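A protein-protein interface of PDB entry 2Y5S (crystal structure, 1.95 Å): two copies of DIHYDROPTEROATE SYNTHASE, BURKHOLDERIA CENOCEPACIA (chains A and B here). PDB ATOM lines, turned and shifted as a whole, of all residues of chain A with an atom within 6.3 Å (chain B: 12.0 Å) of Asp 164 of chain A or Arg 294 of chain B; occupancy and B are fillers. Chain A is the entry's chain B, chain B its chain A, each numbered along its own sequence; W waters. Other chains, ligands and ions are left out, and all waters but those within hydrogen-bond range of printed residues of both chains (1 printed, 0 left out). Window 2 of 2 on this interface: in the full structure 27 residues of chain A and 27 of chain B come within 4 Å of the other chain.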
ATOM      1  N   TYR A 162       6.827  13.910  -9.876  1.00  0.00           N
ATOM      2  CA  TYR A 162       6.181  14.928  -9.040  1.00  0.00           C
ATOM      3  C   TYR A 162       6.938  16.257  -9.086  1.00  0.00           C
ATOM      4  O   TYR A 162       8.115  16.290  -9.391  1.00  0.00           O
ATOM      5  CB  TYR A 162       6.133  14.464  -7.578  1.00  0.00           C
ATOM      6  CG  TYR A 162       5.424  13.149  -7.383  1.00  0.00           C
ATOM      7  CD1 TYR A 162       4.036  13.073  -7.456  1.00  0.00           C
ATOM      8  CD2 TYR A 162       6.134  11.978  -7.163  1.00  0.00           C
ATOM      9  CE1 TYR A 162       3.365  11.869  -7.272  1.00  0.00           C
ATOM     10  CE2 TYR A 162       5.472  10.763  -6.993  1.00  0.00           C
ATOM     11  CZ  TYR A 162       4.082  10.721  -7.055  1.00  0.00           C
ATOM     12  OH  TYR A 162       3.416   9.532  -6.903  1.00  0.00           O
ATOM     13  N   GLY A 163       6.241  17.338  -8.759  1.00  0.00           N
ATOM     14  CA  GLY A 163       6.876  18.610  -8.428  1.00  0.00           C
ATOM     15  C   GLY A 163       7.189  18.512  -6.954  1.00  0.00           C
ATOM     16  O   GLY A 163       8.273  18.067  -6.584  1.00  0.00           O
ATOM     17  N   ASP A 164       6.233  18.896  -6.109  1.00  0.00           N
ATOM     18  CA  ASP A 164       6.273  18.528  -4.698  1.00  0.00           C
ATOM     19  C   ASP A 164       5.267  17.398  -4.492  1.00  0.00           C
ATOM     20  O   ASP A 164       4.061  17.592  -4.640  1.00  0.00           O
ATOM     21  CB  ASP A 164       5.925  19.707  -3.789  1.00  0.00           C
ATOM     22  CG  ASP A 164       5.920  19.330  -2.314  1.00  0.00           C
ATOM     23  OD1 ASP A 164       6.260  18.171  -1.960  1.00  0.00           O
ATOM     24  OD2 ASP A 164       5.581  20.191  -1.482  1.00  0.00           O
ATOM     25  N   VAL A 165       5.770  16.226  -4.146  1.00  0.00           N
ATOM     26  CA  VAL A 165       4.929  15.056  -4.030  1.00  0.00           C
ATOM     27  C   VAL A 165       3.800  15.277  -3.016  1.00  0.00           C
ATOM     28  O   VAL A 165       2.698  14.780  -3.213  1.00  0.00           O
ATOM     29  CB  VAL A 165       5.749  13.793  -3.673  1.00  0.00           C
ATOM     30  CG1 VAL A 165       6.421  13.927  -2.297  1.00  0.00           C
ATOM     31  CG2 VAL A 165       4.858  12.557  -3.729  1.00  0.00           C
ATOM     32  N   VAL A 166       4.068  16.029  -1.947  1.00  0.00           N
ATOM     33  CA  VAL A 166       3.049  16.286  -0.926  1.00  0.00           C
ATOM     34  C   VAL A 166       1.912  17.124  -1.501  1.00  0.00           C
ATOM     35  O   VAL A 166       0.730  16.839  -1.263  1.00  0.00           O
ATOM     36  CB  VAL A 166       3.630  17.013   0.307  1.00  0.00           C
ATOM     37  CG1 VAL A 166       2.530  17.262   1.359  1.00  0.00           C
ATOM     38  CG2 VAL A 166       4.802  16.208   0.912  1.00  0.00           C
ATOM     39  N   THR A 167       2.273  18.161  -2.244  1.00  0.00           N
ATOM     40  CA  THR A 167       1.283  19.032  -2.866  1.00  0.00           C
ATOM     41  C   THR A 167       0.506  18.280  -3.941  1.00  0.00           C
ATOM     42  O   THR A 167      -0.718  18.399  -4.015  1.00  0.00           O
ATOM     43  CB  THR A 167       1.933  20.301  -3.459  1.00  0.00           C
ATOM     44  OG1 THR A 167       2.608  21.009  -2.412  1.00  0.00           O
ATOM     45  CG2 THR A 167       0.881  21.222  -4.089  1.00  0.00           C
ATOM     46  N   ASP A 168       1.208  17.490  -4.756  1.00  0.00           N
ATOM     47  CA  ASP A 168       0.555  16.745  -5.847  1.00  0.00           C
ATOM     48  C   ASP A 168      -0.417  15.719  -5.286  1.00  0.00           C
ATOM     49  O   ASP A 168      -1.506  15.516  -5.830  1.00  0.00           O
ATOM     50  CB  ASP A 168       1.586  16.021  -6.722  1.00  0.00           C
ATOM     51  CG  ASP A 168       2.475  16.977  -7.506  1.00  0.00           C
ATOM     52  OD1 ASP A 168       2.072  18.142  -7.731  1.00  0.00           O
ATOM     53  OD2 ASP A 168       3.582  16.549  -7.901  1.00  0.00           O
ATOM     54  N   VAL A 169      -0.011  15.042  -4.211  1.00  0.00           N
ATOM     55  CA  VAL A 169      -0.866  14.034  -3.584  1.00  0.00           C
ATOM     56  C   VAL A 169      -2.116  14.737  -3.013  1.00  0.00           C
ATOM     57  O   VAL A 169      -3.237  14.286  -3.239  1.00  0.00           O
ATOM     58  CB  VAL A 169      -0.097  13.229  -2.481  1.00  0.00           C
ATOM     59  CG1 VAL A 169      -1.053  12.518  -1.514  1.00  0.00           C
ATOM     60  CG2 VAL A 169       0.865  12.218  -3.125  1.00  0.00           C
ATOM     61  N   ALA A 208       8.964  11.643   2.507  1.00  0.00           N
ATOM     62  CA  ALA A 208       8.465  13.031   2.412  1.00  0.00           C
ATOM     63  C   ALA A 208       6.992  13.053   2.835  1.00  0.00           C
ATOM     64  O   ALA A 208       6.554  13.896   3.618  1.00  0.00           O
ATOM     65  CB  ALA A 208       8.617  13.568   0.987  1.00  0.00           C
ATOM     66  N   ALA A 211       6.742  12.323   6.724  1.00  0.00           N
ATOM     67  CA  ALA A 211       7.171  13.512   7.505  1.00  0.00           C
ATOM     68  C   ALA A 211       6.162  14.667   7.448  1.00  0.00           C
ATOM     69  O   ALA A 211       5.977  15.386   8.436  1.00  0.00           O
ATOM     70  CB  ALA A 211       8.543  14.013   7.022  1.00  0.00           C
ATOM     71  N   ALA A 212       5.532  14.836   6.285  1.00  0.00           N
ATOM     72  CA  ALA A 212       4.551  15.888   6.055  1.00  0.00           C
ATOM     73  C   ALA A 212       3.115  15.387   5.989  1.00  0.00           C
ATOM     74  O   ALA A 212       2.271  16.027   5.372  1.00  0.00           O
ATOM     75  CB  ALA A 212       4.900  16.624   4.763  1.00  0.00           C
ATOM     76  N   ASP A 215      -0.258  17.501   5.824  1.00  0.00           N
ATOM     77  CA  ASP A 215      -0.402  18.313   4.628  1.00  0.00           C
ATOM     78  C   ASP A 215      -0.799  17.528   3.367  1.00  0.00           C
ATOM     79  O   ASP A 215      -1.022  18.137   2.336  1.00  0.00           O
ATOM     80  CB  ASP A 215       0.894  19.081   4.351  1.00  0.00           C
ATOM     81  CG  ASP A 215       1.279  20.018   5.491  1.00  0.00           C
ATOM     82  OD1 ASP A 215       0.368  20.583   6.138  1.00  0.00           O
ATOM     83  OD2 ASP A 215       2.494  20.172   5.735  1.00  0.00           O
ATOM     84  N   THR B   5      15.771  20.953  14.566  1.00  0.00           N
ATOM     85  CA  THR B   5      15.984  19.570  15.063  1.00  0.00           C
ATOM     86  C   THR B   5      16.951  19.572  16.250  1.00  0.00           C
ATOM     87  O   THR B   5      18.039  20.142  16.183  1.00  0.00           O
ATOM     88  CB  THR B   5      16.567  18.638  13.971  1.00  0.00           C
ATOM     89  OG1 THR B   5      15.522  18.174  13.109  1.00  0.00           O
ATOM     90  CG2 THR B   5      17.261  17.433  14.617  1.00  0.00           C
ATOM     91  N   ASN B 285      14.894   7.860  11.742  1.00  0.00           N
ATOM     92  CA  ASN B 285      15.951   8.662  11.090  1.00  0.00           C
ATOM     93  C   ASN B 285      15.574   9.051   9.669  1.00  0.00           C
ATOM     94  O   ASN B 285      15.892  10.153   9.217  1.00  0.00           O
ATOM     95  CB  ASN B 285      17.284   7.908  11.077  1.00  0.00           C
ATOM     96  CG  ASN B 285      18.396   8.648  10.331  1.00  0.00           C
ATOM     97  OD1 ASN B 285      18.949   9.629  10.831  1.00  0.00           O
ATOM     98  ND2 ASN B 285      18.726   8.177   9.121  1.00  0.00           N
ATOM     99  N   ALA B 286      14.907   8.139   8.963  1.00  0.00           N
ATOM    100  CA  ALA B 286      14.506   8.390   7.587  1.00  0.00           C
ATOM    101  C   ALA B 286      13.436   9.478   7.533  1.00  0.00           C
ATOM    102  O   ALA B 286      13.428  10.296   6.612  1.00  0.00           O
ATOM    103  CB  ALA B 286      14.003   7.080   6.904  1.00  0.00           C
ATOM    104  N   VAL B 287      12.539   9.478   8.525  1.00  0.00           N
ATOM    105  CA  VAL B 287      11.496  10.477   8.614  1.00  0.00           C
ATOM    106  C   VAL B 287      12.127  11.837   8.874  1.00  0.00           C
ATOM    107  O   VAL B 287      11.826  12.801   8.180  1.00  0.00           O
ATOM    108  CB  VAL B 287      10.478  10.192   9.741  1.00  0.00           C
ATOM    109  CG1 VAL B 287       9.517  11.396   9.910  1.00  0.00           C
ATOM    110  CG2 VAL B 287       9.672   8.921   9.435  1.00  0.00           C
ATOM    111  N   ARG B 288      13.003  11.891   9.868  1.00  0.00           N
ATOM    112  CA  ARG B 288      13.721  13.131  10.169  1.00  0.00           C
ATOM    113  C   ARG B 288      14.503  13.652   8.969  1.00  0.00           C
ATOM    114  O   ARG B 288      14.500  14.857   8.714  1.00  0.00           O
ATOM    115  CB  ARG B 288      14.639  12.944  11.370  1.00  0.00           C
ATOM    116  CG  ARG B 288      15.232  14.245  11.911  1.00  0.00           C
ATOM    117  CD  ARG B 288      16.192  13.984  13.091  1.00  0.00           C
ATOM    118  NE  ARG B 288      17.373  13.247  12.644  1.00  0.00           N
ATOM    119  CZ  ARG B 288      18.440  12.965  13.393  1.00  0.00           C
ATOM    120  NH1 ARG B 288      18.533  13.385  14.654  1.00  0.00           N
ATOM    121  NH2 ARG B 288      19.433  12.258  12.861  1.00  0.00           N
ATOM    122  N   ALA B 289      15.146  12.764   8.214  1.00  0.00           N
ATOM    123  CA  ALA B 289      15.934  13.197   7.061  1.00  0.00           C
ATOM    124  C   ALA B 289      15.034  13.797   6.007  1.00  0.00           C
ATOM    125  O   ALA B 289      15.389  14.791   5.372  1.00  0.00           O
ATOM    126  CB  ALA B 289      16.752  12.035   6.475  1.00  0.00           C
ATOM    127  N   ALA B 290      13.862  13.197   5.810  1.00  0.00           N
ATOM    128  CA  ALA B 290      12.880  13.770   4.895  1.00  0.00           C
ATOM    129  C   ALA B 290      12.404  15.126   5.416  1.00  0.00           C
ATOM    130  O   ALA B 290      12.308  16.061   4.645  1.00  0.00           O
ATOM    131  CB  ALA B 290      11.692  12.832   4.703  1.00  0.00           C
ATOM    132  N   ALA B 291      12.111  15.224   6.716  1.00  0.00           N
ATOM    133  CA  ALA B 291      11.625  16.488   7.307  1.00  0.00           C
ATOM    134  C   ALA B 291      12.616  17.614   7.049  1.00  0.00           C
ATOM    135  O   ALA B 291      12.220  18.730   6.732  1.00  0.00           O
ATOM    136  CB  ALA B 291      11.388  16.339   8.813  1.00  0.00           C
ATOM    137  N   ARG B 292      13.906  17.293   7.174  1.00  0.00           N
ATOM    138  CA  ARG B 292      14.995  18.260   6.985  1.00  0.00           C
ATOM    139  C   ARG B 292      15.178  18.734   5.557  1.00  0.00           C
ATOM    140  O   ARG B 292      15.936  19.674   5.331  1.00  0.00           O
ATOM    141  CB  ARG B 292      16.325  17.671   7.468  1.00  0.00           C
ATOM    142  CG  ARG B 292      16.387  17.423   8.941  1.00  0.00           C
ATOM    143  CD  ARG B 292      17.659  16.676   9.281  1.00  0.00           C
ATOM    144  NE  ARG B 292      17.905  16.649  10.717  1.00  0.00           N
ATOM    145  CZ  ARG B 292      19.005  16.155  11.277  1.00  0.00           C
ATOM    146  NH1 ARG B 292      19.978  15.636  10.533  1.00  0.00           N
ATOM    147  NH2 ARG B 292      19.133  16.182  12.592  1.00  0.00           N
ATOM    148  N   GLN B 293      14.529  18.080   4.591  1.00  0.00           N
ATOM    149  CA  GLN B 293      14.527  18.564   3.199  1.00  0.00           C
ATOM    150  C   GLN B 293      13.314  19.446   2.881  1.00  0.00           C
ATOM    151  O   GLN B 293      13.137  19.857   1.736  1.00  0.00           O
ATOM    152  CB  GLN B 293      14.560  17.390   2.206  1.00  0.00           C
ATOM    153  CG  GLN B 293      15.811  16.534   2.265  1.00  0.00           C
ATOM    154  CD  GLN B 293      17.084  17.340   2.093  1.00  0.00           C
ATOM    155  OE1 GLN B 293      17.155  18.248   1.259  1.00  0.00           O
ATOM    156  NE2 GLN B 293      18.104  17.010   2.887  1.00  0.00           N
ATOM    157  N   ARG B 294      12.486  19.736   3.882  1.00  0.00           N
ATOM    158  CA  ARG B 294      11.280  20.531   3.678  1.00  0.00           C
ATOM    159  C   ARG B 294      11.379  21.904   4.344  1.00  0.00           C
ATOM    160  O   ARG B 294      12.324  22.211   5.073  1.00  0.00           O
ATOM    161  CB  ARG B 294      10.059  19.764   4.182  1.00  0.00           C
ATOM    162  CG  ARG B 294       9.776  18.533   3.334  1.00  0.00           C
ATOM    163  CD  ARG B 294       8.428  17.897   3.646  1.00  0.00           C
ATOM    164  NE  ARG B 294       7.307  18.716   3.186  1.00  0.00           N
ATOM    165  CZ  ARG B 294       6.906  18.829   1.923  1.00  0.00           C
ATOM    166  NH1 ARG B 294       7.531  18.198   0.933  1.00  0.00           N
ATOM    167  NH2 ARG B 294       5.864  19.597   1.643  1.00  0.00           N
ATOM    168  OXT ARG B 294      10.509  22.750   4.149  1.00  0.00           O
HETATM  169  O   HOH W   1       4.117  20.571   3.597  1.00  0.00           O
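No position is printed for both chains.
Water W1 bridges the side-chain carboxylate of Asp 215 of chain A (2.7 Å) and the guanidinium group of Arg 294 of chain B (2.8 Å).
NH1 of Arg 294 of chain B lies within salt-bridge range of OD1 of Asp 164 of chain A, at 3.2 Å.
Among the printed residues, pairs that only touch across the chains: Val 166 of chain A with Arg 294 of chain B, Ala 208 of chain A with Ala 290 of chain B, Ala 211 of chain A with Val 287 of chain B, Ala 211 of chain A with Ala 291 of chain B and Ala 212 of chain A with Arg 294 of chain B.
Printed residues of chain B that touch a printed residue of chain A: Val 287, Ala 290, Ala 291 and Arg 294.
Hydrophobic or aromatic side chains of chain B within 4 Å of the printed part of chain A: Val 287 and Ala 290.
Among the printed residues, 6 pairs touch across the chains.
Among the printed residues, Asp or Glu carboxylates within 4 Å of a Lys or Arg side-chain nitrogen of the other chain: Asp 164 of chain A with Arg 294 of chain B.
Arg 294 of chain B touches just these residues of chain A: Asp 164, Val 166 and Ala 212.
No residue of chain B comes within 4 Å of Gly 163 of chain A.
No residue of chain B comes within 4 Å of Thr 167 of chain A.
No residue of chain B comes within 4 Å of Asp 168 of chain A.
Ala 208 of chain A touches one residue of chain B.
Of chain B, only Val 287 and Ala 291 come within 4 Å of Ala 211 of chain A.
Of the printed residues of chain A, Ala 291 of chain B touches Ala 211.
Printed residues of chain A within 4 Å of Val 287 of chain B: Ala 211.
Arg 292 of chain B touches none of the printed residues of chain A.
Asn 285 of chain B touches none of the printed residues of chain A.
The nearest residue of chain B that does not touch Asp 164 of chain A is Gln 293 of chain B (8.0 Å).
The nearest residue of chain A that does not touch Arg 294 of chain B is Ala 208 of chain A (4.4 Å).
The nearest printed residue of chain A that does not touch Ala 290 of chain B is Ala 211 of chain A (4.1 Å).
OD2 of Asp 164 of chain A lies within hydrogen-bond range of OG1 of Thr 167 of chain A, at 3.2 Å.
The side-chain carboxylate (OD1) of Asp 164 of chain A sits at hydrogen-bond distance from the backbone NH (N) of Val 166 of chain A (3.1 Å).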
